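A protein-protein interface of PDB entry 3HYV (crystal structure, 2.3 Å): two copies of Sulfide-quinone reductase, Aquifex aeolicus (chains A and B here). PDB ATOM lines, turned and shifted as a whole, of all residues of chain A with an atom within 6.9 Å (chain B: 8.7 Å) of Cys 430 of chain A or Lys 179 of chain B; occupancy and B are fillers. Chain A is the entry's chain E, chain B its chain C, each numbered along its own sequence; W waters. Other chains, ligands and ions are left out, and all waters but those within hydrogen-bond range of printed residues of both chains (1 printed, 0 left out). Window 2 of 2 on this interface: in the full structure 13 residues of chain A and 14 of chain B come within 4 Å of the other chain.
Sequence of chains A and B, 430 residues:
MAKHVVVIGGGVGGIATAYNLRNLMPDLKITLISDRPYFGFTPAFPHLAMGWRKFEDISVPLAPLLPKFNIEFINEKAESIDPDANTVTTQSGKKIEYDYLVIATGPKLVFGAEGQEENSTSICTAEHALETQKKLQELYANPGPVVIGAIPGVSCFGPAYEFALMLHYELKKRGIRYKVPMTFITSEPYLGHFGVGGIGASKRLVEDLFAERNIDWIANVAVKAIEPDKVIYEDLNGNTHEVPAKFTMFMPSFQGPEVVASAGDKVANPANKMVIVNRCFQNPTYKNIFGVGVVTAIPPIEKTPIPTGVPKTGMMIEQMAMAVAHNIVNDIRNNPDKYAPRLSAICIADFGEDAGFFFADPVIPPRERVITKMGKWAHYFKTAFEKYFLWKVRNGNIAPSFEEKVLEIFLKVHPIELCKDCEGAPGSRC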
ATOM      1  N   ARG A 279      25.383   1.641   2.214  1.00  0.00           N
ATOM      2  CA  ARG A 279      24.050   1.039   2.363  1.00  0.00           C
ATOM      3  C   ARG A 279      22.913   2.042   2.192  1.00  0.00           C
ATOM      4  O   ARG A 279      21.825   1.690   1.725  1.00  0.00           O
ATOM      5  CB  ARG A 279      23.915   0.386   3.735  1.00  0.00           C
ATOM      6  CG  ARG A 279      24.661  -0.923   3.885  1.00  0.00           C
ATOM      7  CD  ARG A 279      24.721  -1.288   5.344  1.00  0.00           C
ATOM      8  NE  ARG A 279      25.346  -2.585   5.546  1.00  0.00           N
ATOM      9  CZ  ARG A 279      25.958  -2.953   6.665  1.00  0.00           C
ATOM     10  NH1 ARG A 279      26.494  -4.161   6.754  1.00  0.00           N
ATOM     11  NH2 ARG A 279      26.042  -2.115   7.688  1.00  0.00           N
ATOM     12  N   CYS A 280      23.184   3.284   2.589  1.00  0.00           N
ATOM     13  CA  CYS A 280      22.221   4.374   2.550  1.00  0.00           C
ATOM     14  C   CYS A 280      22.329   5.154   1.234  1.00  0.00           C
ATOM     15  O   CYS A 280      21.750   6.223   1.083  1.00  0.00           O
ATOM     16  CB  CYS A 280      22.419   5.265   3.787  1.00  0.00           C
ATOM     17  SG  CYS A 280      22.134   4.314   5.320  1.00  0.00           S
ATOM     18  N   LYS A 338      18.708   7.367   9.633  1.00  0.00           N
ATOM     19  CA  LYS A 338      19.142   7.116   8.262  1.00  0.00           C
ATOM     20  C   LYS A 338      18.410   5.907   7.683  1.00  0.00           C
ATOM     21  O   LYS A 338      18.017   4.999   8.426  1.00  0.00           O
ATOM     22  CB  LYS A 338      20.641   6.851   8.240  1.00  0.00           C
ATOM     23  CG  LYS A 338      21.514   8.089   8.396  1.00  0.00           C
ATOM     24  CD  LYS A 338      21.918   8.618   7.027  1.00  0.00           C
ATOM     25  CE  LYS A 338      23.356   9.101   7.021  1.00  0.00           C
ATOM     26  NZ  LYS A 338      24.332   7.997   7.243  1.00  0.00           N
ATOM     27  N   TYR A 339      18.253   5.895   6.357  1.00  0.00           N
ATOM     28  CA  TYR A 339      17.449   4.889   5.664  1.00  0.00           C
ATOM     29  C   TYR A 339      18.154   4.178   4.508  1.00  0.00           C
ATOM     30  O   TYR A 339      18.909   4.787   3.742  1.00  0.00           O
ATOM     31  CB  TYR A 339      16.143   5.503   5.152  1.00  0.00           C
ATOM     32  CG  TYR A 339      15.240   5.981   6.254  1.00  0.00           C
ATOM     33  CD1 TYR A 339      14.381   5.100   6.905  1.00  0.00           C
ATOM     34  CD2 TYR A 339      15.250   7.317   6.656  1.00  0.00           C
ATOM     35  CE1 TYR A 339      13.552   5.533   7.929  1.00  0.00           C
ATOM     36  CE2 TYR A 339      14.432   7.758   7.677  1.00  0.00           C
ATOM     37  CZ  TYR A 339      13.585   6.864   8.308  1.00  0.00           C
ATOM     38  OH  TYR A 339      12.771   7.306   9.328  1.00  0.00           O
ATOM     39  N   ALA A 340      17.874   2.884   4.391  1.00  0.00           N
ATOM     40  CA  ALA A 340      18.340   2.070   3.275  1.00  0.00           C
ATOM     41  C   ALA A 340      17.137   1.599   2.444  1.00  0.00           C
ATOM     42  O   ALA A 340      16.081   1.316   3.008  1.00  0.00           O
ATOM     43  CB  ALA A 340      19.133   0.880   3.791  1.00  0.00           C
ATOM     44  N   PRO A 366      19.817 -13.162   0.610  1.00  0.00           N
ATOM     45  CA  PRO A 366      18.670 -14.078   0.716  1.00  0.00           C
ATOM     46  C   PRO A 366      17.325 -13.360   0.580  1.00  0.00           C
ATOM     47  O   PRO A 366      17.182 -12.206   1.011  1.00  0.00           O
ATOM     48  CB  PRO A 366      18.819 -14.664   2.116  1.00  0.00           C
ATOM     49  CG  PRO A 366      19.570 -13.623   2.878  1.00  0.00           C
ATOM     50  CD  PRO A 366      20.521 -13.020   1.897  1.00  0.00           C
ATOM     51  N   ARG A 367      16.355 -14.048  -0.016  1.00  0.00           N
ATOM     52  CA  ARG A 367      15.054 -13.454  -0.308  1.00  0.00           C
ATOM     53  C   ARG A 367      13.980 -13.860   0.694  1.00  0.00           C
ATOM     54  O   ARG A 367      13.986 -14.974   1.213  1.00  0.00           O
ATOM     55  CB  ARG A 367      14.616 -13.791  -1.743  1.00  0.00           C
ATOM     56  CG  ARG A 367      15.663 -13.438  -2.805  1.00  0.00           C
ATOM     57  CD  ARG A 367      15.083 -13.460  -4.197  1.00  0.00           C
ATOM     58  NE  ARG A 367      16.017 -12.932  -5.191  1.00  0.00           N
ATOM     59  CZ  ARG A 367      16.558 -13.639  -6.180  1.00  0.00           C
ATOM     60  NH1 ARG A 367      17.393 -13.055  -7.021  1.00  0.00           N
ATOM     61  NH2 ARG A 367      16.268 -14.924  -6.339  1.00  0.00           N
ATOM     62  N   GLU A 368      13.064 -12.939   0.965  1.00  0.00           N
ATOM     63  CA  GLU A 368      11.865 -13.230   1.755  1.00  0.00           C
ATOM     64  C   GLU A 368      10.822 -13.980   0.914  1.00  0.00           C
ATOM     65  O   GLU A 368      10.162 -14.879   1.428  1.00  0.00           O
ATOM     66  CB  GLU A 368      11.274 -11.937   2.342  1.00  0.00           C
ATOM     67  CG  GLU A 368      10.402 -12.126   3.590  1.00  0.00           C
ATOM     68  CD  GLU A 368      11.193 -12.222   4.900  1.00  0.00           C
ATOM     69  OE1 GLU A 368      12.419 -11.963   4.910  1.00  0.00           O
ATOM     70  OE2 GLU A 368      10.573 -12.552   5.939  1.00  0.00           O
ATOM     71  N   GLU A 417      13.998   0.990   4.871  1.00  0.00           N
ATOM     72  CA  GLU A 417      14.217   0.543   6.251  1.00  0.00           C
ATOM     73  C   GLU A 417      15.154   1.482   7.005  1.00  0.00           C
ATOM     74  O   GLU A 417      16.155   1.944   6.451  1.00  0.00           O
ATOM     75  CB  GLU A 417      14.797  -0.881   6.285  1.00  0.00           C
ATOM     76  CG  GLU A 417      13.963  -1.949   5.551  1.00  0.00           C
ATOM     77  CD  GLU A 417      14.243  -3.390   6.007  1.00  0.00           C
ATOM     78  OE1 GLU A 417      15.178  -3.625   6.813  1.00  0.00           O
ATOM     79  OE2 GLU A 417      13.503  -4.291   5.559  1.00  0.00           O
ATOM     80  N   LEU A 418      14.830   1.749   8.270  1.00  0.00           N
ATOM     81  CA  LEU A 418      15.719   2.479   9.178  1.00  0.00           C
ATOM     82  C   LEU A 418      17.036   1.712   9.369  1.00  0.00           C
ATOM     83  O   LEU A 418      17.030   0.519   9.694  1.00  0.00           O
ATOM     84  CB  LEU A 418      15.022   2.711  10.523  1.00  0.00           C
ATOM     85  CG  LEU A 418      15.614   3.643  11.589  1.00  0.00           C
ATOM     86  CD1 LEU A 418      15.758   5.064  11.078  1.00  0.00           C
ATOM     87  CD2 LEU A 418      14.750   3.620  12.839  1.00  0.00           C
ATOM     88  N   CYS A 419      18.155   2.401   9.137  1.00  0.00           N
ATOM     89  CA  CYS A 419      19.476   1.773   9.126  1.00  0.00           C
ATOM     90  C   CYS A 419      20.381   2.291  10.253  1.00  0.00           C
ATOM     91  O   CYS A 419      20.748   3.460  10.274  1.00  0.00           O
ATOM     92  CB  CYS A 419      20.140   1.949   7.751  1.00  0.00           C
ATOM     93  SG  CYS A 419      21.732   1.081   7.522  1.00  0.00           S
ATOM     94  N   LYS A 420      20.737   1.403  11.178  1.00  0.00           N
ATOM     95  CA  LYS A 420      21.562   1.758  12.344  1.00  0.00           C
ATOM     96  C   LYS A 420      23.061   1.917  12.034  1.00  0.00           C
ATOM     97  O   LYS A 420      23.826   2.363  12.892  1.00  0.00           O
ATOM     98  CB  LYS A 420      21.378   0.724  13.466  1.00  0.00           C
ATOM     99  CG  LYS A 420      21.939  -0.659  13.132  1.00  0.00           C
ATOM    100  CD  LYS A 420      21.778  -1.642  14.285  1.00  0.00           C
ATOM    101  CE  LYS A 420      20.476  -2.430  14.182  1.00  0.00           C
ATOM    102  NZ  LYS A 420      20.404  -3.484  15.245  1.00  0.00           N
ATOM    103  N   ASP A 421      23.469   1.541  10.821  1.00  0.00           N
ATOM    104  CA  ASP A 421      24.873   1.584  10.400  1.00  0.00           C
ATOM    105  C   ASP A 421      24.979   1.473   8.876  1.00  0.00           C
ATOM    106  O   ASP A 421      24.859   0.380   8.319  1.00  0.00           O
ATOM    107  CB  ASP A 421      25.656   0.453  11.087  1.00  0.00           C
ATOM    108  CG  ASP A 421      27.126   0.423  10.703  1.00  0.00           C
ATOM    109  OD1 ASP A 421      27.671   1.469  10.298  1.00  0.00           O
ATOM    110  OD2 ASP A 421      27.743  -0.661  10.817  1.00  0.00           O
ATOM    111  N   CYS A 422      25.204   2.604   8.209  1.00  0.00           N
ATOM    112  CA  CYS A 422      25.289   2.642   6.737  1.00  0.00           C
ATOM    113  C   CYS A 422      26.622   2.113   6.214  1.00  0.00           C
ATOM    114  O   CYS A 422      26.757   1.862   5.019  1.00  0.00           O
ATOM    115  CB  CYS A 422      25.082   4.061   6.186  1.00  0.00           C
ATOM    116  SG  CYS A 422      23.564   4.939   6.646  1.00  0.00           S
ATOM    117  N   SER A 428      23.729  -4.709   1.152  1.00  0.00           N
ATOM    118  CA  SER A 428      23.993  -5.548   2.335  1.00  0.00           C
ATOM    119  C   SER A 428      23.148  -5.096   3.525  1.00  0.00           C
ATOM    120  O   SER A 428      22.694  -3.948   3.582  1.00  0.00           O
ATOM    121  CB  SER A 428      25.491  -5.598   2.700  1.00  0.00           C
ATOM    122  OG  SER A 428      26.002  -4.338   3.097  1.00  0.00           O
ATOM    123  N   ARG A 429      22.942  -5.998   4.476  1.00  0.00           N
ATOM    124  CA  ARG A 429      21.984  -5.761   5.553  1.00  0.00           C
ATOM    125  C   ARG A 429      22.632  -5.055   6.746  1.00  0.00           C
ATOM    126  O   ARG A 429      23.647  -5.533   7.272  1.00  0.00           O
ATOM    127  CB  ARG A 429      21.330  -7.085   5.976  1.00  0.00           C
ATOM    128  CG  ARG A 429      20.115  -7.530   5.130  1.00  0.00           C
ATOM    129  CD  ARG A 429      20.432  -7.790   3.645  1.00  0.00           C
ATOM    130  NE  ARG A 429      19.489  -8.726   3.028  1.00  0.00           N
ATOM    131  CZ  ARG A 429      19.308  -8.887   1.720  1.00  0.00           C
ATOM    132  NH1 ARG A 429      19.993  -8.169   0.844  1.00  0.00           N
ATOM    133  NH2 ARG A 429      18.430  -9.777   1.281  1.00  0.00           N
ATOM    134  N   CYS A 430      22.041  -3.925   7.167  1.00  0.00           N
ATOM    135  CA  CYS A 430      22.569  -3.120   8.295  1.00  0.00           C
ATOM    136  C   CYS A 430      22.632  -3.961   9.562  1.00  0.00           C
ATOM    137  O   CYS A 430      22.030  -5.037   9.646  1.00  0.00           O
ATOM    138  CB  CYS A 430      21.733  -1.843   8.565  1.00  0.00           C
ATOM    139  SG  CYS A 430      21.214  -0.846   7.091  1.00  0.00           S
ATOM    140  OXT CYS A 430      23.285  -3.585  10.537  1.00  0.00           O
ATOM    141  N   LEU B 139      20.469 -17.610  17.188  1.00  0.00           N
ATOM    142  CA  LEU B 139      20.415 -17.227  15.779  1.00  0.00           C
ATOM    143  C   LEU B 139      19.424 -16.090  15.525  1.00  0.00           C
ATOM    144  O   LEU B 139      19.768 -15.123  14.849  1.00  0.00           O
ATOM    145  CB  LEU B 139      20.079 -18.438  14.893  1.00  0.00           C
ATOM    146  CG  LEU B 139      19.951 -18.237  13.375  1.00  0.00           C
ATOM    147  CD1 LEU B 139      21.294 -17.854  12.738  1.00  0.00           C
ATOM    148  CD2 LEU B 139      19.371 -19.496  12.705  1.00  0.00           C
ATOM    149  N   TYR B 140      18.204 -16.217  16.056  1.00  0.00           N
ATOM    150  CA  TYR B 140      17.164 -15.193  15.884  1.00  0.00           C
ATOM    151  C   TYR B 140      17.591 -13.835  16.449  1.00  0.00           C
ATOM    152  O   TYR B 140      17.210 -12.795  15.908  1.00  0.00           O
ATOM    153  CB  TYR B 140      15.820 -15.618  16.520  1.00  0.00           C
ATOM    154  CG  TYR B 140      15.308 -17.007  16.153  1.00  0.00           C
ATOM    155  CD1 TYR B 140      15.434 -17.511  14.854  1.00  0.00           C
ATOM    156  CD2 TYR B 140      14.663 -17.802  17.104  1.00  0.00           C
ATOM    157  CE1 TYR B 140      14.952 -18.780  14.521  1.00  0.00           C
ATOM    158  CE2 TYR B 140      14.184 -19.072  16.784  1.00  0.00           C
ATOM    159  CZ  TYR B 140      14.330 -19.550  15.489  1.00  0.00           C
ATOM    160  OH  TYR B 140      13.861 -20.795  15.158  1.00  0.00           O
ATOM    161  N   ALA B 141      18.371 -13.851  17.531  1.00  0.00           N
ATOM    162  CA  ALA B 141      18.862 -12.620  18.166  1.00  0.00           C
ATOM    163  C   ALA B 141      19.928 -11.889  17.330  1.00  0.00           C
ATOM    164  O   ALA B 141      19.906 -10.658  17.244  1.00  0.00           O
ATOM    165  CB  ALA B 141      19.379 -12.904  19.577  1.00  0.00           C
ATOM    166  N   ASN B 142      20.864 -12.641  16.743  1.00  0.00           N
ATOM    167  CA  ASN B 142      21.773 -12.093  15.731  1.00  0.00           C
ATOM    168  C   ASN B 142      21.964 -13.011  14.525  1.00  0.00           C
ATOM    169  O   ASN B 142      22.857 -13.858  14.521  1.00  0.00           O
ATOM    170  CB  ASN B 142      23.124 -11.623  16.319  1.00  0.00           C
ATOM    171  CG  ASN B 142      23.706 -12.587  17.338  1.00  0.00           C
ATOM    172  OD1 ASN B 142      23.689 -13.807  17.153  1.00  0.00           O
ATOM    173  ND2 ASN B 142      24.243 -12.032  18.427  1.00  0.00           N
ATOM    174  N   PRO B 143      21.096 -12.858  13.504  1.00  0.00           N
ATOM    175  CA  PRO B 143      21.116 -13.675  12.284  1.00  0.00           C
ATOM    176  C   PRO B 143      22.484 -13.816  11.599  1.00  0.00           C
ATOM    177  O   PRO B 143      23.388 -12.996  11.804  1.00  0.00           O
ATOM    178  CB  PRO B 143      20.116 -12.963  11.353  1.00  0.00           C
ATOM    179  CG  PRO B 143      19.680 -11.721  12.056  1.00  0.00           C
ATOM    180  CD  PRO B 143      19.978 -11.897  13.499  1.00  0.00           C
ATOM    181  N   GLY B 144      22.606 -14.869  10.793  1.00  0.00           N
ATOM    182  CA  GLY B 144      23.793 -15.134   9.992  1.00  0.00           C
ATOM    183  C   GLY B 144      23.574 -16.317   9.052  1.00  0.00           C
ATOM    184  O   GLY B 144      22.507 -16.940   9.077  1.00  0.00           O
ATOM    185  N   PRO B 145      24.585 -16.635   8.220  1.00  0.00           N
ATOM    186  CA  PRO B 145      24.504 -17.742   7.262  1.00  0.00           C
ATOM    187  C   PRO B 145      24.201 -19.094   7.913  1.00  0.00           C
ATOM    188  O   PRO B 145      24.785 -19.437   8.937  1.00  0.00           O
ATOM    189  CB  PRO B 145      25.890 -17.753   6.597  1.00  0.00           C
ATOM    190  CG  PRO B 145      26.763 -16.928   7.477  1.00  0.00           C
ATOM    191  CD  PRO B 145      25.873 -15.927   8.141  1.00  0.00           C
ATOM    192  N   VAL B 146      23.269 -19.833   7.313  1.00  0.00           N
ATOM    193  CA  VAL B 146      22.862 -21.158   7.789  1.00  0.00           C
ATOM    194  C   VAL B 146      23.197 -22.183   6.711  1.00  0.00           C
ATOM    195  O   VAL B 146      22.947 -21.938   5.524  1.00  0.00           O
ATOM    196  CB  VAL B 146      21.336 -21.199   8.127  1.00  0.00           C
ATOM    197  CG1 VAL B 146      20.825 -22.631   8.274  1.00  0.00           C
ATOM    198  CG2 VAL B 146      21.042 -20.406   9.393  1.00  0.00           C
ATOM    199  N   LEU B 171      11.644 -18.383  10.260  1.00  0.00           N
ATOM    200  CA  LEU B 171      12.380 -17.156   9.966  1.00  0.00           C
ATOM    201  C   LEU B 171      11.487 -16.140   9.251  1.00  0.00           C
ATOM    202  O   LEU B 171      11.555 -14.938   9.514  1.00  0.00           O
ATOM    203  CB  LEU B 171      13.592 -17.482   9.095  1.00  0.00           C
ATOM    204  CG  LEU B 171      15.035 -17.557   9.619  1.00  0.00           C
ATOM    205  CD1 LEU B 171      15.192 -17.655  11.129  1.00  0.00           C
ATOM    206  CD2 LEU B 171      15.797 -18.646   8.881  1.00  0.00           C
ATOM    207  N   ARG B 174       8.822 -14.527  11.546  1.00  0.00           N
ATOM    208  CA  ARG B 174       9.399 -13.454  12.347  1.00  0.00           C
ATOM    209  C   ARG B 174      10.008 -12.302  11.511  1.00  0.00           C
ATOM    210  O   ARG B 174      10.581 -11.362  12.060  1.00  0.00           O
ATOM    211  CB  ARG B 174      10.314 -13.968  13.483  1.00  0.00           C
ATOM    212  CG  ARG B 174      11.404 -14.951  13.116  1.00  0.00           C
ATOM    213  CD  ARG B 174      12.174 -15.376  14.366  1.00  0.00           C
ATOM    214  NE  ARG B 174      11.438 -16.310  15.222  1.00  0.00           N
ATOM    215  CZ  ARG B 174      11.445 -16.293  16.558  1.00  0.00           C
ATOM    216  NH1 ARG B 174      12.125 -15.368  17.228  1.00  0.00           N
ATOM    217  NH2 ARG B 174      10.749 -17.199  17.237  1.00  0.00           N
ATOM    218  N   GLY B 175       9.839 -12.382  10.189  1.00  0.00           N
ATOM    219  CA  GLY B 175      10.215 -11.306   9.259  1.00  0.00           C
ATOM    220  C   GLY B 175      11.707 -11.075   9.093  1.00  0.00           C
ATOM    221  O   GLY B 175      12.140  -9.964   8.785  1.00  0.00           O
ATOM    222  N   ILE B 176      12.484 -12.140   9.245  1.00  0.00           N
ATOM    223  CA  ILE B 176      13.934 -12.056   9.388  1.00  0.00           C
ATOM    224  C   ILE B 176      14.690 -12.918   8.343  1.00  0.00           C
ATOM    225  O   ILE B 176      15.920 -12.893   8.272  1.00  0.00           O
ATOM    226  CB  ILE B 176      14.303 -12.327  10.900  1.00  0.00           C
ATOM    227  CG1 ILE B 176      14.571 -10.999  11.617  1.00  0.00           C
ATOM    228  CG2 ILE B 176      15.441 -13.344  11.098  1.00  0.00           C
ATOM    229  CD1 ILE B 176      14.605 -11.107  13.131  1.00  0.00           C
ATOM    230  N   ARG B 177      13.939 -13.631   7.502  1.00  0.00           N
ATOM    231  CA  ARG B 177      14.513 -14.531   6.483  1.00  0.00           C
ATOM    232  C   ARG B 177      15.515 -13.843   5.530  1.00  0.00           C
ATOM    233  O   ARG B 177      16.507 -14.455   5.119  1.00  0.00           O
ATOM    234  CB  ARG B 177      13.388 -15.264   5.712  1.00  0.00           C
ATOM    235  CG  ARG B 177      13.824 -16.156   4.535  1.00  0.00           C
ATOM    236  CD  ARG B 177      14.627 -17.392   4.973  1.00  0.00           C
ATOM    237  NE  ARG B 177      15.911 -17.432   4.276  1.00  0.00           N
ATOM    238  CZ  ARG B 177      16.149 -18.068   3.132  1.00  0.00           C
ATOM    239  NH1 ARG B 177      15.206 -18.774   2.530  1.00  0.00           N
ATOM    240  NH2 ARG B 177      17.357 -18.004   2.595  1.00  0.00           N
ATOM    241  N   TYR B 178      15.266 -12.569   5.217  1.00  0.00           N
ATOM    242  CA  TYR B 178      16.107 -11.792   4.302  1.00  0.00           C
ATOM    243  C   TYR B 178      17.463 -11.441   4.913  1.00  0.00           C
ATOM    244  O   TYR B 178      18.341 -10.891   4.238  1.00  0.00           O
ATOM    245  CB  TYR B 178      15.364 -10.526   3.809  1.00  0.00           C
ATOM    246  CG  TYR B 178      15.289  -9.387   4.812  1.00  0.00           C
ATOM    247  CD1 TYR B 178      16.036  -8.220   4.631  1.00  0.00           C
ATOM    248  CD2 TYR B 178      14.474  -9.477   5.940  1.00  0.00           C
ATOM    249  CE1 TYR B 178      15.966  -7.164   5.555  1.00  0.00           C
ATOM    250  CE2 TYR B 178      14.400  -8.444   6.866  1.00  0.00           C
ATOM    251  CZ  TYR B 178      15.145  -7.290   6.669  1.00  0.00           C
ATOM    252  OH  TYR B 178      15.061  -6.276   7.594  1.00  0.00           O
ATOM    253  N   LYS B 179      17.619 -11.757   6.195  1.00  0.00           N
ATOM    254  CA  LYS B 179      18.883 -11.569   6.907  1.00  0.00           C
ATOM    255  C   LYS B 179      19.628 -12.895   7.086  1.00  0.00           C
ATOM    256  O   LYS B 179      20.754 -12.913   7.590  1.00  0.00           O
ATOM    257  CB  LYS B 179      18.633 -10.945   8.283  1.00  0.00           C
ATOM    258  CG  LYS B 179      18.141  -9.508   8.270  1.00  0.00           C
ATOM    259  CD  LYS B 179      17.962  -9.020   9.698  1.00  0.00           C
ATOM    260  CE  LYS B 179      17.670  -7.530   9.767  1.00  0.00           C
ATOM    261  NZ  LYS B 179      18.873  -6.703   9.453  1.00  0.00           N
ATOM    262  N   VAL B 180      19.001 -14.000   6.684  1.00  0.00           N
ATOM    263  CA  VAL B 180      19.585 -15.337   6.867  1.00  0.00           C
ATOM    264  C   VAL B 180      19.781 -16.112   5.546  1.00  0.00           C
ATOM    265  O   VAL B 180      18.817 -16.674   5.008  1.00  0.00           O
ATOM    266  CB  VAL B 180      18.744 -16.199   7.868  1.00  0.00           C
ATOM    267  CG1 VAL B 180      19.367 -17.578   8.065  1.00  0.00           C
ATOM    268  CG2 VAL B 180      18.597 -15.491   9.206  1.00  0.00           C
ATOM    269  N   PRO B 181      21.027 -16.147   5.023  1.00  0.00           N
ATOM    270  CA  PRO B 181      21.371 -17.083   3.947  1.00  0.00           C
ATOM    271  C   PRO B 181      21.116 -18.548   4.334  1.00  0.00           C
ATOM    272  O   PRO B 181      21.350 -18.933   5.478  1.00  0.00           O
ATOM    273  CB  PRO B 181      22.875 -16.839   3.727  1.00  0.00           C
ATOM    274  CG  PRO B 181      23.110 -15.421   4.201  1.00  0.00           C
ATOM    275  CD  PRO B 181      22.169 -15.273   5.380  1.00  0.00           C
ATOM    276  N   MET B 182      20.619 -19.338   3.383  1.00  0.00           N
ATOM    277  CA  MET B 182      20.323 -20.761   3.595  1.00  0.00           C
ATOM    278  C   MET B 182      20.902 -21.615   2.461  1.00  0.00           C
ATOM    279  O   MET B 182      20.598 -21.387   1.294  1.00  0.00           O
ATOM    280  CB  MET B 182      18.802 -21.003   3.743  1.00  0.00           C
ATOM    281  CG  MET B 182      18.175 -20.397   5.017  1.00  0.00           C
ATOM    282  SD  MET B 182      16.547 -21.037   5.520  1.00  0.00           S
ATOM    283  CE  MET B 182      16.986 -22.706   6.053  1.00  0.00           C
ATOM    284  N   LYS B 246      27.185 -19.549  10.357  1.00  0.00           N
ATOM    285  CA  LYS B 246      27.081 -19.202  11.783  1.00  0.00           C
ATOM    286  C   LYS B 246      26.345 -20.276  12.596  1.00  0.00           C
ATOM    287  O   LYS B 246      26.639 -20.489  13.777  1.00  0.00           O
ATOM    288  CB  LYS B 246      26.348 -17.872  11.940  1.00  0.00           C
ATOM    289  CG  LYS B 246      26.748 -17.072  13.158  1.00  0.00           C
ATOM    290  CD  LYS B 246      25.713 -15.995  13.466  1.00  0.00           C
ATOM    291  CE  LYS B 246      24.722 -16.459  14.542  1.00  0.00           C
ATOM    292  NZ  LYS B 246      25.062 -15.887  15.884  1.00  0.00           N
HETATM  293  O   HOH W   1      17.308  -4.268   8.904  1.00  0.00           O
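The backbone NH (N) of Arg 177 of chain B lies within hydrogen-bond range of the side-chain carboxylate (OE1) of Glu 368 of chain A.
The side-chain carboxylate (OE1) of Glu 368 of chain A is in hydrogen-bond range of the backbone NH (N) of Tyr 178 of chain B, at 2.9 Å.
OH of Tyr 178 of chain B sits at hydrogen-bond distance from OE1 of Glu 417 of chain A (2.8 Å).
The guanidinium group (NE) of Arg 429 of chain A is in hydrogen-bond range of the backbone carbonyl oxygen (O) of Tyr 178 of chain B, at 2.7 Å.
NZ of Lys 179 of chain B is in salt-bridge range of O of Cys 430 of chain A.
N of Val 146 of chain B sits at hydrogen-bond distance from O of Pro 181 of chain B (2.8 Å).
The backbone NH (N) of Arg 177 of chain B sits at hydrogen-bond distance from the backbone carbonyl oxygen (O) of Leu 171 of chain B (3.4 Å).
The backbone carbonyl oxygen (O) of Val 180 of chain B is in hydrogen-bond range of the guanidinium group (NE) of Arg 177 of chain B (3.1 Å).
The backbone carbonyl oxygen (O) of Arg 429 of chain A sits at hydrogen-bond distance from the guanidinium group (NH1) of Arg 279 of chain A (3.2 Å).
The guanidinium group (NH2) of Arg 429 of chain A sits at hydrogen-bond distance from the backbone carbonyl oxygen (O) of Pro 366 of chain A, at 2.7 Å.
SG of Cys 430 of chain A forms a disulfide with SG of Cys 419 of chain A, at 2.0 Å.
Pro 366 of chain A touches Arg 177 of chain B.
Pro 366 of chain A touches Tyr 178 of chain B.
CB of Pro 366 of chain A touches O of Val 180 of chain B (3.5 Å).
CG of Pro 366 of chain A touches N of Pro 181 of chain B, 3.6 Å away.
Arg 177 of chain B touches Arg 367 of chain A (CG to O, 3.5 Å).
CA of Gly 175 of chain B touches OE2 of Glu 368 of chain A (3.6 Å).
Ile 176 of chain B touches Glu 368 of chain A (N to OE2, 3.8 Å).
Of the printed residues of chain B, Cys 430 of chain A touches Lys 179 (3.6 Å).
Of the printed residues of chain A, Ile 176 of chain B touches Glu 368 (3.8 Å).
Of the printed residues of chain A, Arg 177 of chain B touches Pro 366 (3.7 Å), Arg 367 (3.5 Å) and Glu 368 (3.4 Å).
Printed residues of chain A within 4 Å of Val 180 of chain B: Pro 366 (3.5 Å).
Of the printed residues of chain B, Arg 367 of chain A touches Arg 177.
Of the 19 printed residues of chain B, 7 touch a printed residue of chain A.
Printed residues of chain B that touch a printed residue of chain A: Gly 175, Ile 176, Arg 177, Tyr 178, Lys 179, Val 180 and Pro 181.
Hydrophobic or aromatic side chains of chain B within 4 Å of the printed part of chain A: Tyr 178 and Pro 181.
Among the printed residues, 12 pairs touch across the chains.
Among the printed residues, no Asp or Glu carboxylate lies within 4 Å of a Lys or Arg side-chain nitrogen of the other chain.
No position is printed for both chains.
Water W1 lies within hydrogen-bond range of NZ of Lys 179 of chain B, OE1 of Glu 417 of chain A and OH of Tyr 178 of chain B.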
